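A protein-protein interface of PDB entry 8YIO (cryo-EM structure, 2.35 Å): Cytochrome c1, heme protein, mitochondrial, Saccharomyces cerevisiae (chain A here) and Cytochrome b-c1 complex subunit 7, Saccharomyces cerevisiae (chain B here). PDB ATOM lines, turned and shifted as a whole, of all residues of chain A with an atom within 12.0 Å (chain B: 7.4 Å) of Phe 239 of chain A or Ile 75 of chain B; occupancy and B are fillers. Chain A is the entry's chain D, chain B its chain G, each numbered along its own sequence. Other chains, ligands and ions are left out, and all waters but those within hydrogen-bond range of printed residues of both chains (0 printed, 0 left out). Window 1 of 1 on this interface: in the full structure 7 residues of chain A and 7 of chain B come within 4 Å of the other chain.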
ATOM      1  N   TRP A 231       6.739  -4.238 -12.578  1.00  0.00           N
ATOM      2  CA  TRP A 231       7.746  -5.287 -12.596  1.00  0.00           C
ATOM      3  C   TRP A 231       7.270  -6.557 -13.284  1.00  0.00           C
ATOM      4  O   TRP A 231       8.042  -7.514 -13.379  1.00  0.00           O
ATOM      5  CB  TRP A 231       8.193  -5.621 -11.163  1.00  0.00           C
ATOM      6  CG  TRP A 231       9.402  -4.860 -10.702  1.00  0.00           C
ATOM      7  CD1 TRP A 231       9.436  -3.576 -10.254  1.00  0.00           C
ATOM      8  CD2 TRP A 231      10.750  -5.338 -10.647  1.00  0.00           C
ATOM      9  NE1 TRP A 231      10.716  -3.221  -9.924  1.00  0.00           N
ATOM     10  CE2 TRP A 231      11.544  -4.286 -10.156  1.00  0.00           C
ATOM     11  CE3 TRP A 231      11.364  -6.554 -10.965  1.00  0.00           C
ATOM     12  CZ2 TRP A 231      12.920  -4.410  -9.975  1.00  0.00           C
ATOM     13  CZ3 TRP A 231      12.727  -6.675 -10.787  1.00  0.00           C
ATOM     14  CH2 TRP A 231      13.491  -5.610 -10.296  1.00  0.00           C
ATOM     15  N   ALA A 232       6.030  -6.589 -13.779  1.00  0.00           N
ATOM     16  CA  ALA A 232       5.437  -7.830 -14.266  1.00  0.00           C
ATOM     17  C   ALA A 232       6.032  -8.301 -15.587  1.00  0.00           C
ATOM     18  O   ALA A 232       5.974  -9.498 -15.878  1.00  0.00           O
ATOM     19  CB  ALA A 232       3.923  -7.666 -14.405  1.00  0.00           C
ATOM     20  N   GLY A 233       6.603  -7.400 -16.386  1.00  0.00           N
ATOM     21  CA  GLY A 233       7.256  -7.825 -17.613  1.00  0.00           C
ATOM     22  C   GLY A 233       8.563  -8.558 -17.365  1.00  0.00           C
ATOM     23  O   GLY A 233       8.912  -9.485 -18.099  1.00  0.00           O
ATOM     24  N   ILE A 234       9.300  -8.153 -16.331  1.00  0.00           N
ATOM     25  CA  ILE A 234      10.555  -8.814 -15.987  1.00  0.00           C
ATOM     26  C   ILE A 234      10.290 -10.165 -15.326  1.00  0.00           C
ATOM     27  O   ILE A 234      10.987 -11.152 -15.596  1.00  0.00           O
ATOM     28  CB  ILE A 234      11.402  -7.887 -15.092  1.00  0.00           C
ATOM     29  CG1 ILE A 234      11.729  -6.585 -15.828  1.00  0.00           C
ATOM     30  CG2 ILE A 234      12.681  -8.563 -14.623  1.00  0.00           C
ATOM     31  CD1 ILE A 234      12.707  -6.744 -16.966  1.00  0.00           C
ATOM     32  N   LYS A 235       9.258 -10.243 -14.483  1.00  0.00           N
ATOM     33  CA  LYS A 235       9.017 -11.441 -13.683  1.00  0.00           C
ATOM     34  C   LYS A 235       8.494 -12.620 -14.498  1.00  0.00           C
ATOM     35  O   LYS A 235       8.606 -13.761 -14.039  1.00  0.00           O
ATOM     36  CB  LYS A 235       8.034 -11.130 -12.553  1.00  0.00           C
ATOM     37  CG  LYS A 235       8.569 -10.175 -11.506  1.00  0.00           C
ATOM     38  CD  LYS A 235       9.016 -10.892 -10.248  1.00  0.00           C
ATOM     39  CE  LYS A 235       9.724  -9.931  -9.306  1.00  0.00           C
ATOM     40  NZ  LYS A 235       9.835 -10.467  -7.925  1.00  0.00           N
ATOM     41  N   THR A 236       7.934 -12.388 -15.685  1.00  0.00           N
ATOM     42  CA  THR A 236       7.400 -13.469 -16.507  1.00  0.00           C
ATOM     43  C   THR A 236       8.227 -13.704 -17.768  1.00  0.00           C
ATOM     44  O   THR A 236       7.758 -14.360 -18.699  1.00  0.00           O
ATOM     45  CB  THR A 236       5.937 -13.197 -16.864  1.00  0.00           C
ATOM     46  OG1 THR A 236       5.790 -11.844 -17.304  1.00  0.00           O
ATOM     47  CG2 THR A 236       5.052 -13.418 -15.656  1.00  0.00           C
ATOM     48  N   ARG A 237       9.455 -13.199 -17.796  1.00  0.00           N
ATOM     49  CA  ARG A 237      10.348 -13.348 -18.938  1.00  0.00           C
ATOM     50  C   ARG A 237      10.853 -14.787 -19.064  1.00  0.00           C
ATOM     51  O   ARG A 237      11.115 -15.457 -18.063  1.00  0.00           O
ATOM     52  CB  ARG A 237      11.508 -12.372 -18.768  1.00  0.00           C
ATOM     53  CG  ARG A 237      12.446 -12.215 -19.924  1.00  0.00           C
ATOM     54  CD  ARG A 237      13.417 -11.086 -19.631  1.00  0.00           C
ATOM     55  NE  ARG A 237      13.950 -11.166 -18.276  1.00  0.00           N
ATOM     56  CZ  ARG A 237      14.956 -10.428 -17.818  1.00  0.00           C
ATOM     57  NH1 ARG A 237      15.375 -10.577 -16.570  1.00  0.00           N
ATOM     58  NH2 ARG A 237      15.544  -9.543 -18.606  1.00  0.00           N
ATOM     59  N   LYS A 238      10.984 -15.269 -20.305  1.00  0.00           N
ATOM     60  CA  LYS A 238      11.384 -16.643 -20.587  1.00  0.00           C
ATOM     61  C   LYS A 238      12.601 -16.687 -21.506  1.00  0.00           C
ATOM     62  O   LYS A 238      12.758 -15.841 -22.386  1.00  0.00           O
ATOM     63  CB  LYS A 238      10.232 -17.432 -21.223  1.00  0.00           C
ATOM     64  CG  LYS A 238       8.981 -17.460 -20.375  1.00  0.00           C
ATOM     65  CD  LYS A 238       7.905 -18.319 -20.979  1.00  0.00           C
ATOM     66  CE  LYS A 238       6.594 -18.123 -20.250  1.00  0.00           C
ATOM     67  NZ  LYS A 238       6.740 -18.319 -18.783  1.00  0.00           N
ATOM     68  N   PHE A 239      13.455 -17.698 -21.308  1.00  0.00           N
ATOM     69  CA  PHE A 239      14.697 -17.863 -22.059  1.00  0.00           C
ATOM     70  C   PHE A 239      14.765 -19.248 -22.689  1.00  0.00           C
ATOM     71  O   PHE A 239      14.292 -20.226 -22.109  1.00  0.00           O
ATOM     72  CB  PHE A 239      15.930 -17.660 -21.167  1.00  0.00           C
ATOM     73  CG  PHE A 239      16.142 -16.242 -20.725  1.00  0.00           C
ATOM     74  CD1 PHE A 239      16.888 -15.366 -21.493  1.00  0.00           C
ATOM     75  CD2 PHE A 239      15.609 -15.788 -19.528  1.00  0.00           C
ATOM     76  CE1 PHE A 239      17.091 -14.060 -21.082  1.00  0.00           C
ATOM     77  CE2 PHE A 239      15.808 -14.485 -19.113  1.00  0.00           C
ATOM     78  CZ  PHE A 239      16.550 -13.621 -19.891  1.00  0.00           C
ATOM     79  N   VAL A 240      15.369 -19.328 -23.876  1.00  0.00           N
ATOM     80  CA  VAL A 240      15.519 -20.572 -24.630  1.00  0.00           C
ATOM     81  C   VAL A 240      16.933 -20.610 -25.206  1.00  0.00           C
ATOM     82  O   VAL A 240      17.407 -19.616 -25.765  1.00  0.00           O
ATOM     83  CB  VAL A 240      14.446 -20.684 -25.743  1.00  0.00           C
ATOM     84  CG1 VAL A 240      14.825 -21.692 -26.809  1.00  0.00           C
ATOM     85  CG2 VAL A 240      13.092 -21.054 -25.165  1.00  0.00           C
ATOM     86  N   PHE A 241      17.614 -21.747 -25.064  1.00  0.00           N
ATOM     87  CA  PHE A 241      18.972 -21.924 -25.564  1.00  0.00           C
ATOM     88  C   PHE A 241      19.005 -22.933 -26.704  1.00  0.00           C
ATOM     89  O   PHE A 241      18.536 -24.064 -26.551  1.00  0.00           O
ATOM     90  CB  PHE A 241      19.912 -22.381 -24.448  1.00  0.00           C
ATOM     91  CG  PHE A 241      21.353 -22.475 -24.864  1.00  0.00           C
ATOM     92  CD1 PHE A 241      21.979 -21.410 -25.489  1.00  0.00           C
ATOM     93  CD2 PHE A 241      22.082 -23.626 -24.618  1.00  0.00           C
ATOM     94  CE1 PHE A 241      23.309 -21.492 -25.868  1.00  0.00           C
ATOM     95  CE2 PHE A 241      23.411 -23.717 -24.994  1.00  0.00           C
ATOM     96  CZ  PHE A 241      24.026 -22.648 -25.618  1.00  0.00           C
ATOM     97  N   ASN A 242      19.567 -22.523 -27.834  1.00  0.00           N
ATOM     98  CA  ASN A 242      19.879 -23.423 -28.938  1.00  0.00           C
ATOM     99  C   ASN A 242      21.381 -23.370 -29.180  1.00  0.00           C
ATOM    100  O   ASN A 242      21.910 -22.284 -29.470  1.00  0.00           O
ATOM    101  CB  ASN A 242      19.116 -23.037 -30.208  1.00  0.00           C
ATOM    102  CG  ASN A 242      17.633 -23.315 -30.108  1.00  0.00           C
ATOM    103  OD1 ASN A 242      16.840 -22.421 -29.821  1.00  0.00           O
ATOM    104  ND2 ASN A 242      17.250 -24.557 -30.344  1.00  0.00           N
ATOM    105  N   PRO A 243      22.105 -24.482 -29.056  1.00  0.00           N
ATOM    106  CA  PRO A 243      23.576 -24.447 -29.179  1.00  0.00           C
ATOM    107  C   PRO A 243      24.014 -24.133 -30.597  1.00  0.00           C
ATOM    108  O   PRO A 243      23.514 -24.735 -31.559  1.00  0.00           O
ATOM    109  CB  PRO A 243      24.002 -25.865 -28.766  1.00  0.00           C
ATOM    110  CG  PRO A 243      22.844 -26.416 -28.017  1.00  0.00           C
ATOM    111  CD  PRO A 243      21.624 -25.801 -28.619  1.00  0.00           C
ATOM    112  N   LEU B  42      23.127 -24.951 -11.844  1.00  0.00           N
ATOM    113  CA  LEU B  42      24.521 -24.538 -11.894  1.00  0.00           C
ATOM    114  C   LEU B  42      25.451 -25.701 -11.577  1.00  0.00           C
ATOM    115  O   LEU B  42      25.111 -26.605 -10.813  1.00  0.00           O
ATOM    116  CB  LEU B  42      24.792 -23.388 -10.918  1.00  0.00           C
ATOM    117  CG  LEU B  42      24.096 -22.045 -11.157  1.00  0.00           C
ATOM    118  CD1 LEU B  42      24.041 -21.227  -9.874  1.00  0.00           C
ATOM    119  CD2 LEU B  42      24.764 -21.252 -12.277  1.00  0.00           C
ATOM    120  N   ALA B  69      27.624 -22.243 -23.329  1.00  0.00           N
ATOM    121  CA  ALA B  69      26.762 -22.977 -22.410  1.00  0.00           C
ATOM    122  C   ALA B  69      26.888 -22.469 -20.980  1.00  0.00           C
ATOM    123  O   ALA B  69      25.923 -22.543 -20.215  1.00  0.00           O
ATOM    124  CB  ALA B  69      27.080 -24.470 -22.475  1.00  0.00           C
ATOM    125  N   ARG B  70      28.066 -21.963 -20.603  1.00  0.00           N
ATOM    126  CA  ARG B  70      28.249 -21.377 -19.279  1.00  0.00           C
ATOM    127  C   ARG B  70      27.455 -20.083 -19.135  1.00  0.00           C
ATOM    128  O   ARG B  70      26.896 -19.808 -18.068  1.00  0.00           O
ATOM    129  CB  ARG B  70      29.741 -21.143 -19.021  1.00  0.00           C
ATOM    130  CG  ARG B  70      30.083 -20.416 -17.728  1.00  0.00           C
ATOM    131  CD  ARG B  70      31.543 -19.996 -17.686  1.00  0.00           C
ATOM    132  NE  ARG B  70      31.868 -19.237 -16.482  1.00  0.00           N
ATOM    133  CZ  ARG B  70      31.903 -17.910 -16.413  1.00  0.00           C
ATOM    134  NH1 ARG B  70      32.201 -17.315 -15.272  1.00  0.00           N
ATOM    135  NH2 ARG B  70      31.639 -17.177 -17.480  1.00  0.00           N
ATOM    136  N   ALA B  71      27.372 -19.292 -20.208  1.00  0.00           N
ATOM    137  CA  ALA B  71      26.638 -18.031 -20.163  1.00  0.00           C
ATOM    138  C   ALA B  71      25.134 -18.245 -20.035  1.00  0.00           C
ATOM    139  O   ALA B  71      24.452 -17.437 -19.399  1.00  0.00           O
ATOM    140  CB  ALA B  71      26.952 -17.200 -21.405  1.00  0.00           C
ATOM    141  N   TYR B  72      24.605 -19.327 -20.609  1.00  0.00           N
ATOM    142  CA  TYR B  72      23.176 -19.601 -20.500  1.00  0.00           C
ATOM    143  C   TYR B  72      22.796 -20.073 -19.096  1.00  0.00           C
ATOM    144  O   TYR B  72      21.716 -19.738 -18.599  1.00  0.00           O
ATOM    145  CB  TYR B  72      22.754 -20.629 -21.552  1.00  0.00           C
ATOM    146  CG  TYR B  72      21.362 -21.167 -21.345  1.00  0.00           C
ATOM    147  CD1 TYR B  72      20.253 -20.340 -21.466  1.00  0.00           C
ATOM    148  CD2 TYR B  72      21.154 -22.496 -21.003  1.00  0.00           C
ATOM    149  CE1 TYR B  72      18.979 -20.822 -21.266  1.00  0.00           C
ATOM    150  CE2 TYR B  72      19.881 -22.989 -20.802  1.00  0.00           C
ATOM    151  CZ  TYR B  72      18.798 -22.144 -20.934  1.00  0.00           C
ATOM    152  OH  TYR B  72      17.530 -22.623 -20.735  1.00  0.00           O
ATOM    153  N   ARG B  73      23.673 -20.839 -18.436  1.00  0.00           N
ATOM    154  CA  ARG B  73      23.371 -21.335 -17.094  1.00  0.00           C
ATOM    155  C   ARG B  73      23.378 -20.209 -16.062  1.00  0.00           C
ATOM    156  O   ARG B  73      22.586 -20.227 -15.117  1.00  0.00           O
ATOM    157  CB  ARG B  73      24.364 -22.433 -16.698  1.00  0.00           C
ATOM    158  CG  ARG B  73      24.175 -23.756 -17.428  1.00  0.00           C
ATOM    159  CD  ARG B  73      25.004 -24.893 -16.825  1.00  0.00           C
ATOM    160  NE  ARG B  73      26.419 -24.556 -16.699  1.00  0.00           N
ATOM    161  CZ  ARG B  73      27.362 -24.894 -17.574  1.00  0.00           C
ATOM    162  NH1 ARG B  73      28.617 -24.534 -17.366  1.00  0.00           N
ATOM    163  NH2 ARG B  73      27.054 -25.590 -18.656  1.00  0.00           N
ATOM    164  N   ILE B  74      24.254 -19.220 -16.238  1.00  0.00           N
ATOM    165  CA  ILE B  74      24.322 -18.092 -15.314  1.00  0.00           C
ATOM    166  C   ILE B  74      23.098 -17.192 -15.471  1.00  0.00           C
ATOM    167  O   ILE B  74      22.523 -16.724 -14.481  1.00  0.00           O
ATOM    168  CB  ILE B  74      25.650 -17.335 -15.526  1.00  0.00           C
ATOM    169  CG1 ILE B  74      26.810 -18.131 -14.925  1.00  0.00           C
ATOM    170  CG2 ILE B  74      25.619 -15.928 -14.933  1.00  0.00           C
ATOM    171  CD1 ILE B  74      28.178 -17.545 -15.198  1.00  0.00           C
ATOM    172  N   ILE B  75      22.654 -16.976 -16.713  1.00  0.00           N
ATOM    173  CA  ILE B  75      21.501 -16.122 -16.984  1.00  0.00           C
ATOM    174  C   ILE B  75      20.213 -16.775 -16.486  1.00  0.00           C
ATOM    175  O   ILE B  75      19.358 -16.111 -15.887  1.00  0.00           O
ATOM    176  CB  ILE B  75      21.449 -15.788 -18.490  1.00  0.00           C
ATOM    177  CG1 ILE B  75      22.494 -14.727 -18.834  1.00  0.00           C
ATOM    178  CG2 ILE B  75      20.073 -15.313 -18.935  1.00  0.00           C
ATOM    179  CD1 ILE B  75      22.704 -14.536 -20.312  1.00  0.00           C
ATOM    180  N   ARG B  76      20.073 -18.090 -16.691  1.00  0.00           N
ATOM    181  CA  ARG B  76      18.900 -18.819 -16.211  1.00  0.00           C
ATOM    182  C   ARG B  76      18.834 -18.856 -14.683  1.00  0.00           C
ATOM    183  O   ARG B  76      17.739 -18.836 -14.114  1.00  0.00           O
ATOM    184  CB  ARG B  76      18.900 -20.239 -16.795  1.00  0.00           C
ATOM    185  CG  ARG B  76      17.699 -21.106 -16.415  1.00  0.00           C
ATOM    186  CD  ARG B  76      17.755 -22.507 -17.013  1.00  0.00           C
ATOM    187  NE  ARG B  76      18.926 -23.260 -16.581  1.00  0.00           N
ATOM    188  CZ  ARG B  76      19.230 -24.483 -17.002  1.00  0.00           C
ATOM    189  NH1 ARG B  76      20.319 -25.086 -16.555  1.00  0.00           N
ATOM    190  NH2 ARG B  76      18.446 -25.103 -17.866  1.00  0.00           N
ATOM    191  N   ALA B  77      19.984 -18.864 -14.004  1.00  0.00           N
ATOM    192  CA  ALA B  77      19.988 -18.865 -12.545  1.00  0.00           C
ATOM    193  C   ALA B  77      19.617 -17.506 -11.959  1.00  0.00           C
ATOM    194  O   ALA B  77      19.053 -17.448 -10.864  1.00  0.00           O
ATOM    195  CB  ALA B  77      21.354 -19.309 -12.018  1.00  0.00           C
ATOM    196  N   HIS B  78      19.918 -16.411 -12.662  1.00  0.00           N
ATOM    197  CA  HIS B  78      19.511 -15.092 -12.189  1.00  0.00           C
ATOM    198  C   HIS B  78      18.005 -14.889 -12.322  1.00  0.00           C
ATOM    199  O   HIS B  78      17.383 -14.258 -11.463  1.00  0.00           O
ATOM    200  CB  HIS B  78      20.257 -14.000 -12.951  1.00  0.00           C
ATOM    201  CG  HIS B  78      21.607 -13.679 -12.392  1.00  0.00           C
ATOM    202  ND1 HIS B  78      22.768 -13.828 -13.118  1.00  0.00           N
ATOM    203  CD2 HIS B  78      21.982 -13.213 -11.179  1.00  0.00           C
ATOM    204  CE1 HIS B  78      23.799 -13.470 -12.375  1.00  0.00           C
ATOM    205  NE2 HIS B  78      23.349 -13.092 -11.194  1.00  0.00           N
ATOM    206  N   GLN B  79      17.405 -15.414 -13.395  1.00  0.00           N
ATOM    207  CA  GLN B  79      15.969 -15.261 -13.608  1.00  0.00           C
ATOM    208  C   GLN B  79      15.164 -16.110 -12.634  1.00  0.00           C
ATOM    209  O   GLN B  79      14.107 -15.676 -12.168  1.00  0.00           O
ATOM    210  CB  GLN B  79      15.618 -15.606 -15.062  1.00  0.00           C
ATOM    211  CG  GLN B  79      14.132 -15.537 -15.424  1.00  0.00           C
ATOM    212  CD  GLN B  79      13.575 -14.123 -15.412  1.00  0.00           C
ATOM    213  OE1 GLN B  79      14.273 -13.167 -15.729  1.00  0.00           O
ATOM    214  NE2 GLN B  79      12.311 -13.991 -15.050  1.00  0.00           N
ATOM    215  N   THR B  80      15.658 -17.302 -12.296  1.00  0.00           N
ATOM    216  CA  THR B  80      14.988 -18.152 -11.317  1.00  0.00           C
ATOM    217  C   THR B  80      15.068 -17.560  -9.914  1.00  0.00           C
ATOM    218  O   THR B  80      14.140 -17.724  -9.117  1.00  0.00           O
ATOM    219  CB  THR B  80      15.607 -19.555 -11.348  1.00  0.00           C
ATOM    220  OG1 THR B  80      15.761 -19.975 -12.706  1.00  0.00           O
ATOM    221  CG2 THR B  80      14.730 -20.561 -10.639  1.00  0.00           C
ATOM    222  N   GLU B  81      16.155 -16.847  -9.613  1.00  0.00           N
ATOM    223  CA  GLU B  81      16.351 -16.277  -8.285  1.00  0.00           C
ATOM    224  C   GLU B  81      15.400 -15.114  -8.023  1.00  0.00           C
ATOM    225  O   GLU B  81      14.870 -14.982  -6.914  1.00  0.00           O
ATOM    226  CB  GLU B  81      17.811 -15.845  -8.134  1.00  0.00           C
ATOM    227  CG  GLU B  81      18.153 -15.094  -6.860  1.00  0.00           C
ATOM    228  CD  GLU B  81      18.145 -15.978  -5.632  1.00  0.00           C
ATOM    229  OE1 GLU B  81      17.941 -15.448  -4.522  1.00  0.00           O
ATOM    230  OE2 GLU B  81      18.345 -17.202  -5.771  1.00  0.00           O
ATOM    231  N   LEU B  82      15.150 -14.270  -9.029  1.00  0.00           N
ATOM    232  CA  LEU B  82      14.277 -13.120  -8.818  1.00  0.00           C
ATOM    233  C   LEU B  82      12.800 -13.495  -8.752  1.00  0.00           C
ATOM    234  O   LEU B  82      12.008 -12.715  -8.218  1.00  0.00           O
ATOM    235  CB  LEU B  82      14.508 -12.056  -9.901  1.00  0.00           C
ATOM    236  CG  LEU B  82      14.134 -12.232 -11.379  1.00  0.00           C
ATOM    237  CD1 LEU B  82      12.774 -11.640 -11.709  1.00  0.00           C
ATOM    238  CD2 LEU B  82      15.199 -11.597 -12.252  1.00  0.00           C
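Of chain A, only Phe 239 (3.9 Å) comes within 4 Å of Ile 75 of chain B. No residue of chain A comes within 4 Å of Ala 71 of chain B. Of chain A, only Phe 241 (3.6 Å) comes within 4 Å of Tyr 72 of chain B. Ala 77 of chain B touches none of the printed residues of chain A. No residue of chain A comes within 4 Å of His 78 of chain B. Printed residues of chain B within 4 Å of Arg 237 of chain A: Gln 79. Printed residues of chain A within 4 Å of Leu 82 of chain B: Lys 235 (3.1 Å). Of the printed residues of chain B, Lys 235 of chain A touches Gln 79 (3.8 Å) and Leu 82 (3.1 Å). Thr 80 of chain B touches none of the printed residues of chain A. The nearest residue of chain B that does not touch Phe 239 of chain A is Tyr 72 of chain B (4.3 Å). The nearest residue of chain A that does not touch Ile 75 of chain B is Arg 237 of chain A (6.9 Å). The nearest printed residue of chain A that does not touch Leu 82 of chain B is Ile 234 of chain A (4.2 Å).
Printed residues of chain B that touch a printed residue of chain A: Tyr 72, Ile 75, Gln 79 and Leu 82. Hydrophobic or aromatic side chains of chain B within 4 Å of the printed part of chain A: Tyr 72 and Ile 75. Of the 13 printed residues of chain A, 5 touch a printed residue of chain B. Hydrophobic or aromatic side chains of chain A that line the printed part of chain B: Phe 239 and Phe 241. Among the printed residues, no Asp or Glu carboxylate lies within 4 Å of a Lys or Arg side-chain nitrogen of the other chain.
NE2 of Gln 79 of chain B is in hydrogen-bond range of O of Ile 234 of chain A (3.2 Å). The side-chain amino group of Lys 235 of chain A is in hydrogen-bond range of the backbone carbonyl oxygen of Leu 82 of chain B (3.1 Å). The side-chain amide oxygen (OE1) of Gln 79 of chain B sits at hydrogen-bond distance from the guanidinium group (NH1) of Arg 237 of chain A, 2.9 Å away.
Lys 235 of chain A touches Gln 79 of chain B (O to NE2, 3.8 Å). Ile 75 of chain B touches Phe 239 of chain A (CG2 to CE1, 3.9 Å). Phe 239 of chain A touches Gln 79 of chain B (CE2 to OE1, 3.9 Å). Phe 241 of chain A touches Tyr 72 of chain B (CB to CD1, 3.6 Å).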
